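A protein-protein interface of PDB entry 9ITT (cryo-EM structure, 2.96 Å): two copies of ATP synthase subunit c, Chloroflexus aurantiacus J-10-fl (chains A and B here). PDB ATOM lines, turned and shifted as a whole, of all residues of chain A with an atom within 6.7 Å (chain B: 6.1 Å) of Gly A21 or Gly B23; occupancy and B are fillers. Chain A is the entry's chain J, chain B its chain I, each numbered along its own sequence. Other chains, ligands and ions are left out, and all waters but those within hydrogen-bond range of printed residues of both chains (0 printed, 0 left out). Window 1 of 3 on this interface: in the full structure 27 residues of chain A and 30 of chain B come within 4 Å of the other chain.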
ATOM      1  N   GLY A  16      14.463   2.077  30.940  1.00  0.00           N
ATOM      2  CA  GLY A  16      13.266   2.564  30.278  1.00  0.00           C
ATOM      3  C   GLY A  16      13.316   4.035  29.936  1.00  0.00           C
ATOM      4  O   GLY A  16      12.500   4.501  29.135  1.00  0.00           O
ATOM      5  N   ALA A  17      14.236   4.784  30.546  1.00  0.00           N
ATOM      6  CA  ALA A  17      14.459   6.176  30.175  1.00  0.00           C
ATOM      7  C   ALA A  17      15.536   6.338  29.111  1.00  0.00           C
ATOM      8  O   ALA A  17      15.538   7.346  28.394  1.00  0.00           O
ATOM      9  CB  ALA A  17      14.844   6.994  31.411  1.00  0.00           C
ATOM     10  N   ILE A  18      16.455   5.376  28.998  1.00  0.00           N
ATOM     11  CA  ILE A  18      17.566   5.513  28.055  1.00  0.00           C
ATOM     12  C   ILE A  18      17.052   5.594  26.619  1.00  0.00           C
ATOM     13  O   ILE A  18      17.426   6.494  25.858  1.00  0.00           O
ATOM     14  CB  ILE A  18      18.565   4.354  28.238  1.00  0.00           C
ATOM     15  CG1 ILE A  18      19.520   4.672  29.389  1.00  0.00           C
ATOM     16  CG2 ILE A  18      19.368   4.087  26.952  1.00  0.00           C
ATOM     17  CD1 ILE A  18      20.277   3.477  29.913  1.00  0.00           C
ATOM     18  N   GLY A  19      16.195   4.656  26.228  1.00  0.00           N
ATOM     19  CA  GLY A  19      15.781   4.535  24.848  1.00  0.00           C
ATOM     20  C   GLY A  19      14.783   5.585  24.411  1.00  0.00           C
ATOM     21  O   GLY A  19      15.001   6.315  23.438  1.00  0.00           O
ATOM     22  N   PRO A  20      13.648   5.658  25.111  1.00  0.00           N
ATOM     23  CA  PRO A  20      12.606   6.615  24.712  1.00  0.00           C
ATOM     24  C   PRO A  20      13.076   8.055  24.661  1.00  0.00           C
ATOM     25  O   PRO A  20      12.569   8.824  23.838  1.00  0.00           O
ATOM     26  CB  PRO A  20      11.526   6.405  25.779  1.00  0.00           C
ATOM     27  CG  PRO A  20      11.668   4.974  26.140  1.00  0.00           C
ATOM     28  CD  PRO A  20      13.145   4.694  26.105  1.00  0.00           C
ATOM     29  N   GLY A  21      14.031   8.452  25.504  1.00  0.00           N
ATOM     30  CA  GLY A  21      14.583   9.792  25.384  1.00  0.00           C
ATOM     31  C   GLY A  21      15.237  10.018  24.035  1.00  0.00           C
ATOM     32  O   GLY A  21      14.976  11.018  23.359  1.00  0.00           O
ATOM     33  N   VAL A  22      16.080   9.073  23.612  1.00  0.00           N
ATOM     34  CA  VAL A  22      16.734   9.179  22.311  1.00  0.00           C
ATOM     35  C   VAL A  22      15.700   9.156  21.193  1.00  0.00           C
ATOM     36  O   VAL A  22      15.806   9.902  20.211  1.00  0.00           O
ATOM     37  CB  VAL A  22      17.767   8.049  22.139  1.00  0.00           C
ATOM     38  CG1 VAL A  22      18.399   8.110  20.752  1.00  0.00           C
ATOM     39  CG2 VAL A  22      18.840   8.133  23.212  1.00  0.00           C
ATOM     40  N   GLY A  23      14.701   8.280  21.310  1.00  0.00           N
ATOM     41  CA  GLY A  23      13.680   8.207  20.279  1.00  0.00           C
ATOM     42  C   GLY A  23      12.911   9.506  20.137  1.00  0.00           C
ATOM     43  O   GLY A  23      12.721  10.013  19.028  1.00  0.00           O
ATOM     44  N   ILE A  24      12.474  10.073  21.264  1.00  0.00           N
ATOM     45  CA  ILE A  24      11.758  11.344  21.238  1.00  0.00           C
ATOM     46  C   ILE A  24      12.650  12.433  20.667  1.00  0.00           C
ATOM     47  O   ILE A  24      12.191  13.304  19.917  1.00  0.00           O
ATOM     48  CB  ILE A  24      11.264  11.705  22.652  1.00  0.00           C
ATOM     49  CG1 ILE A  24      10.134  10.764  23.073  1.00  0.00           C
ATOM     50  CG2 ILE A  24      10.798  13.163  22.702  1.00  0.00           C
ATOM     51  CD1 ILE A  24       9.817  10.804  24.550  1.00  0.00           C
ATOM     52  N   GLY A  25      13.936  12.411  21.019  1.00  0.00           N
ATOM     53  CA  GLY A  25      14.836  13.423  20.502  1.00  0.00           C
ATOM     54  C   GLY A  25      14.972  13.355  18.996  1.00  0.00           C
ATOM     55  O   GLY A  25      14.895  14.374  18.305  1.00  0.00           O
ATOM     56  N   ILE A  26      15.163  12.145  18.466  1.00  0.00           N
ATOM     57  CA  ILE A  26      15.268  11.977  17.021  1.00  0.00           C
ATOM     58  C   ILE A  26      13.970  12.404  16.346  1.00  0.00           C
ATOM     59  O   ILE A  26      13.983  13.052  15.290  1.00  0.00           O
ATOM     60  CB  ILE A  26      15.639  10.522  16.677  1.00  0.00           C
ATOM     61  CG1 ILE A  26      17.068  10.218  17.143  1.00  0.00           C
ATOM     62  CG2 ILE A  26      15.492  10.275  15.178  1.00  0.00           C
ATOM     63  CD1 ILE A  26      17.420   8.742  17.154  1.00  0.00           C
ATOM     64  N   VAL A  28      11.718  14.636  17.374  1.00  0.00           N
ATOM     65  CA  VAL A  28      11.553  16.084  17.388  1.00  0.00           C
ATOM     66  C   VAL A  28      12.545  16.744  16.441  1.00  0.00           C
ATOM     67  O   VAL A  28      12.212  17.716  15.756  1.00  0.00           O
ATOM     68  CB  VAL A  28      11.688  16.616  18.825  1.00  0.00           C
ATOM     69  CG1 VAL A  28      11.757  18.140  18.831  1.00  0.00           C
ATOM     70  CG2 VAL A  28      10.524  16.129  19.676  1.00  0.00           C
ATOM     71  N   THR A  56       6.807   6.378  21.299  1.00  0.00           N
ATOM     72  CA  THR A  56       8.107   6.308  21.960  1.00  0.00           C
ATOM     73  C   THR A  56       7.960   6.356  23.477  1.00  0.00           C
ATOM     74  O   THR A  56       8.618   5.594  24.194  1.00  0.00           O
ATOM     75  CB  THR A  56       9.001   7.447  21.472  1.00  0.00           C
ATOM     76  OG1 THR A  56       9.006   7.475  20.039  1.00  0.00           O
ATOM     77  CG2 THR A  56      10.420   7.262  21.972  1.00  0.00           C
ATOM     78  N   GLU A  57       7.100   7.244  23.982  1.00  0.00           N
ATOM     79  CA  GLU A  57       6.853   7.342  25.415  1.00  0.00           C
ATOM     80  C   GLU A  57       6.164   6.101  25.963  1.00  0.00           C
ATOM     81  O   GLU A  57       6.177   5.889  27.180  1.00  0.00           O
ATOM     82  CB  GLU A  57       6.003   8.585  25.704  1.00  0.00           C
ATOM     83  CG  GLU A  57       5.923   9.004  27.177  1.00  0.00           C
ATOM     84  CD  GLU A  57       7.040   9.944  27.603  1.00  0.00           C
ATOM     85  OE1 GLU A  57       7.908  10.276  26.770  1.00  0.00           O
ATOM     86  OE2 GLU A  57       7.046  10.357  28.782  1.00  0.00           O
ATOM     87  N   ALA A  60       8.723   3.999  27.757  1.00  0.00           N
ATOM     88  CA  ALA A  60       9.088   4.627  29.023  1.00  0.00           C
ATOM     89  C   ALA A  60       8.008   4.407  30.070  1.00  0.00           C
ATOM     90  O   ALA A  60       8.308   4.125  31.236  1.00  0.00           O
ATOM     91  CB  ALA A  60       9.329   6.123  28.820  1.00  0.00           C
ATOM     92  N   ILE B  18      20.815   9.462  30.879  1.00  0.00           N
ATOM     93  CA  ILE B  18      21.449   9.208  29.588  1.00  0.00           C
ATOM     94  C   ILE B  18      20.501   9.550  28.444  1.00  0.00           C
ATOM     95  O   ILE B  18      20.776  10.434  27.622  1.00  0.00           O
ATOM     96  CB  ILE B  18      21.924   7.743  29.507  1.00  0.00           C
ATOM     97  CG1 ILE B  18      23.181   7.555  30.365  1.00  0.00           C
ATOM     98  CG2 ILE B  18      22.175   7.328  28.044  1.00  0.00           C
ATOM     99  CD1 ILE B  18      23.643   6.113  30.509  1.00  0.00           C
ATOM    100  N   GLY B  19      19.373   8.847  28.378  1.00  0.00           N
ATOM    101  CA  GLY B  19      18.434   8.996  27.295  1.00  0.00           C
ATOM    102  C   GLY B  19      17.893  10.403  27.170  1.00  0.00           C
ATOM    103  O   GLY B  19      17.862  10.975  26.079  1.00  0.00           O
ATOM    104  N   PRO B  20      17.432  10.983  28.282  1.00  0.00           N
ATOM    105  CA  PRO B  20      17.012  12.391  28.235  1.00  0.00           C
ATOM    106  C   PRO B  20      18.113  13.339  27.799  1.00  0.00           C
ATOM    107  O   PRO B  20      17.834  14.292  27.065  1.00  0.00           O
ATOM    108  CB  PRO B  20      16.563  12.666  29.675  1.00  0.00           C
ATOM    109  CG  PRO B  20      16.100  11.350  30.170  1.00  0.00           C
ATOM    110  CD  PRO B  20      17.002  10.327  29.529  1.00  0.00           C
ATOM    111  N   GLY B  21      19.359  13.108  28.217  1.00  0.00           N
ATOM    112  CA  GLY B  21      20.437  13.985  27.786  1.00  0.00           C
ATOM    113  C   GLY B  21      20.653  13.936  26.286  1.00  0.00           C
ATOM    114  O   GLY B  21      20.713  14.973  25.615  1.00  0.00           O
ATOM    115  N   VAL B  22      20.745  12.725  25.733  1.00  0.00           N
ATOM    116  CA  VAL B  22      20.942  12.596  24.293  1.00  0.00           C
ATOM    117  C   VAL B  22      19.728  13.129  23.540  1.00  0.00           C
ATOM    118  O   VAL B  22      19.862  13.734  22.469  1.00  0.00           O
ATOM    119  CB  VAL B  22      21.251  11.135  23.919  1.00  0.00           C
ATOM    120  CG1 VAL B  22      21.498  11.008  22.419  1.00  0.00           C
ATOM    121  CG2 VAL B  22      22.462  10.631  24.694  1.00  0.00           C
ATOM    122  N   GLY B  23      18.528  12.923  24.086  1.00  0.00           N
ATOM    123  CA  GLY B  23      17.337  13.431  23.433  1.00  0.00           C
ATOM    124  C   GLY B  23      17.301  14.944  23.388  1.00  0.00           C
ATOM    125  O   GLY B  23      16.988  15.535  22.354  1.00  0.00           O
ATOM    126  N   ILE B  24      17.625  15.593  24.511  1.00  0.00           N
ATOM    127  CA  ILE B  24      17.704  17.050  24.537  1.00  0.00           C
ATOM    128  C   ILE B  24      18.746  17.535  23.543  1.00  0.00           C
ATOM    129  O   ILE B  24      18.540  18.529  22.833  1.00  0.00           O
ATOM    130  CB  ILE B  24      18.019  17.550  25.961  1.00  0.00           C
ATOM    131  CG1 ILE B  24      16.864  17.237  26.914  1.00  0.00           C
ATOM    132  CG2 ILE B  24      18.309  19.048  25.946  1.00  0.00           C
ATOM    133  CD1 ILE B  24      17.253  17.257  28.380  1.00  0.00           C
ATOM    134  N   GLY B  25      19.887  16.846  23.479  1.00  0.00           N
ATOM    135  CA  GLY B  25      20.920  17.256  22.547  1.00  0.00           C
ATOM    136  C   GLY B  25      20.456  17.191  21.106  1.00  0.00           C
ATOM    137  O   GLY B  25      20.656  18.129  20.329  1.00  0.00           O
ATOM    138  N   ILE B  26      19.813  16.082  20.734  1.00  0.00           N
ATOM    139  CA  ILE B  26      19.329  15.928  19.365  1.00  0.00           C
ATOM    140  C   ILE B  26      18.238  16.952  19.071  1.00  0.00           C
ATOM    141  O   ILE B  26      18.173  17.512  17.969  1.00  0.00           O
ATOM    142  CB  ILE B  26      18.842  14.485  19.129  1.00  0.00           C
ATOM    143  CG1 ILE B  26      20.024  13.510  19.232  1.00  0.00           C
ATOM    144  CG2 ILE B  26      18.164  14.381  17.764  1.00  0.00           C
ATOM    145  CD1 ILE B  26      19.640  12.040  19.193  1.00  0.00           C
ATOM    146  N   ILE B  27      17.369  17.218  20.052  1.00  0.00           N
ATOM    147  CA  ILE B  27      16.318  18.220  19.882  1.00  0.00           C
ATOM    148  C   ILE B  27      16.930  19.572  19.564  1.00  0.00           C
ATOM    149  O   ILE B  27      16.534  20.251  18.607  1.00  0.00           O
ATOM    150  CB  ILE B  27      15.446  18.303  21.149  1.00  0.00           C
ATOM    151  CG1 ILE B  27      14.587  17.058  21.288  1.00  0.00           C
ATOM    152  CG2 ILE B  27      14.559  19.540  21.118  1.00  0.00           C
ATOM    153  CD1 ILE B  27      14.157  16.761  22.707  1.00  0.00           C
ATOM    154  N   VAL B  28      17.900  19.988  20.376  1.00  0.00           N
ATOM    155  CA  VAL B  28      18.490  21.308  20.205  1.00  0.00           C
ATOM    156  C   VAL B  28      19.251  21.381  18.889  1.00  0.00           C
ATOM    157  O   VAL B  28      19.199  22.397  18.190  1.00  0.00           O
ATOM    158  CB  VAL B  28      19.382  21.640  21.413  1.00  0.00           C
ATOM    159  CG1 VAL B  28      20.307  22.815  21.108  1.00  0.00           C
ATOM    160  CG2 VAL B  28      18.522  21.934  22.631  1.00  0.00           C
ATOM    161  N   THR B  56      11.609  15.124  27.543  1.00  0.00           N
ATOM    162  CA  THR B  56      12.846  14.511  28.020  1.00  0.00           C
ATOM    163  C   THR B  56      13.104  14.860  29.482  1.00  0.00           C
ATOM    164  O   THR B  56      13.517  14.001  30.273  1.00  0.00           O
ATOM    165  CB  THR B  56      14.020  14.958  27.151  1.00  0.00           C
ATOM    166  OG1 THR B  56      14.072  16.390  27.121  1.00  0.00           O
ATOM    167  CG2 THR B  56      13.874  14.424  25.732  1.00  0.00           C
ATOM    168  N   LEU B  59      10.924  12.743  31.695  1.00  0.00           N
ATOM    169  CA  LEU B  59      11.507  11.417  31.896  1.00  0.00           C
ATOM    170  C   LEU B  59      12.659  11.472  32.897  1.00  0.00           C
ATOM    171  O   LEU B  59      12.769  10.615  33.791  1.00  0.00           O
ATOM    172  CB  LEU B  59      11.982  10.845  30.560  1.00  0.00           C
ATOM    173  CG  LEU B  59      10.906  10.591  29.500  1.00  0.00           C
ATOM    174  CD1 LEU B  59      11.544  10.121  28.202  1.00  0.00           C
ATOM    175  CD2 LEU B  59       9.880   9.577  29.987  1.00  0.00           C
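Of the 15 printed residues of chain A, 9 touch a printed residue of chain B.
Hydrophobic or aromatic side chains of chain A within 4 Å of the printed part of chain B: Ile A18, Val A22, Ile A26, Val A28 and Ala A60.
Of the 13 printed residues of chain B, 8 touch a printed residue of chain A.
Among the printed residues, merely in contact across the chains: Ile A18 with Gly B19, Glu A57 with Leu B59, Gly A25 with Ile B26, Gly A21 with Gly B23, Gly A21 with Gly B19, Ala A17 with Gly B19, Ala A17 with Pro B20, Gly A25 with Gly B23, Val A22 with Gly B19, Ala A60 with Leu B59, Gly A25 with Ile B27, Ile A26 with Ile B26, Val A28 with Ile B27, Ile A18 with Ile B18 and Val A22 with Val B22.
Gly A21 touches just these residues of chain B: Gly B19 (3.5 Å) and Gly B23 (3.4 Å).
Gly B23 touches two residues of chain A.
Of the printed residues of chain B, Ile A26 touches Ile B26.
Of the printed residues of chain A, Ile B26 touches Gly A25 and Ile A26.
Printed residues of chain B within 4 Å of Val A22: Gly B19 and Val B22.
Printed residues of chain A within 4 Å of Ile B27: Gly A25 (3.7 Å) and Val A28 (3.8 Å).
The nearest residue of chain B that does not touch Gly A21 is Leu B59 (4.03 Å).
The nearest residue of chain A that does not touch Gly B23 is Val A22 (4.4 Å).
Ile A18 touches Gly B19, but with the chains exchanged Gly A19 does not touch Ile B18 (6.8 Å).
Gly A21 touches Gly B19, but with the chains exchanged Gly A19 does not touch Gly B21 (9.2 Å).
Gly A21 touches Gly B23, but with the chains exchanged Gly A23 does not touch Gly B21 (9.6 Å).
Gly A25 touches Ile B26, but with the chains exchanged Ile A26 does not touch Gly B25 (7.8 Å).
Of the 15 pairs that touch across the chains among the printed residues, 3 have their exchanged pair printed and touching as well.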
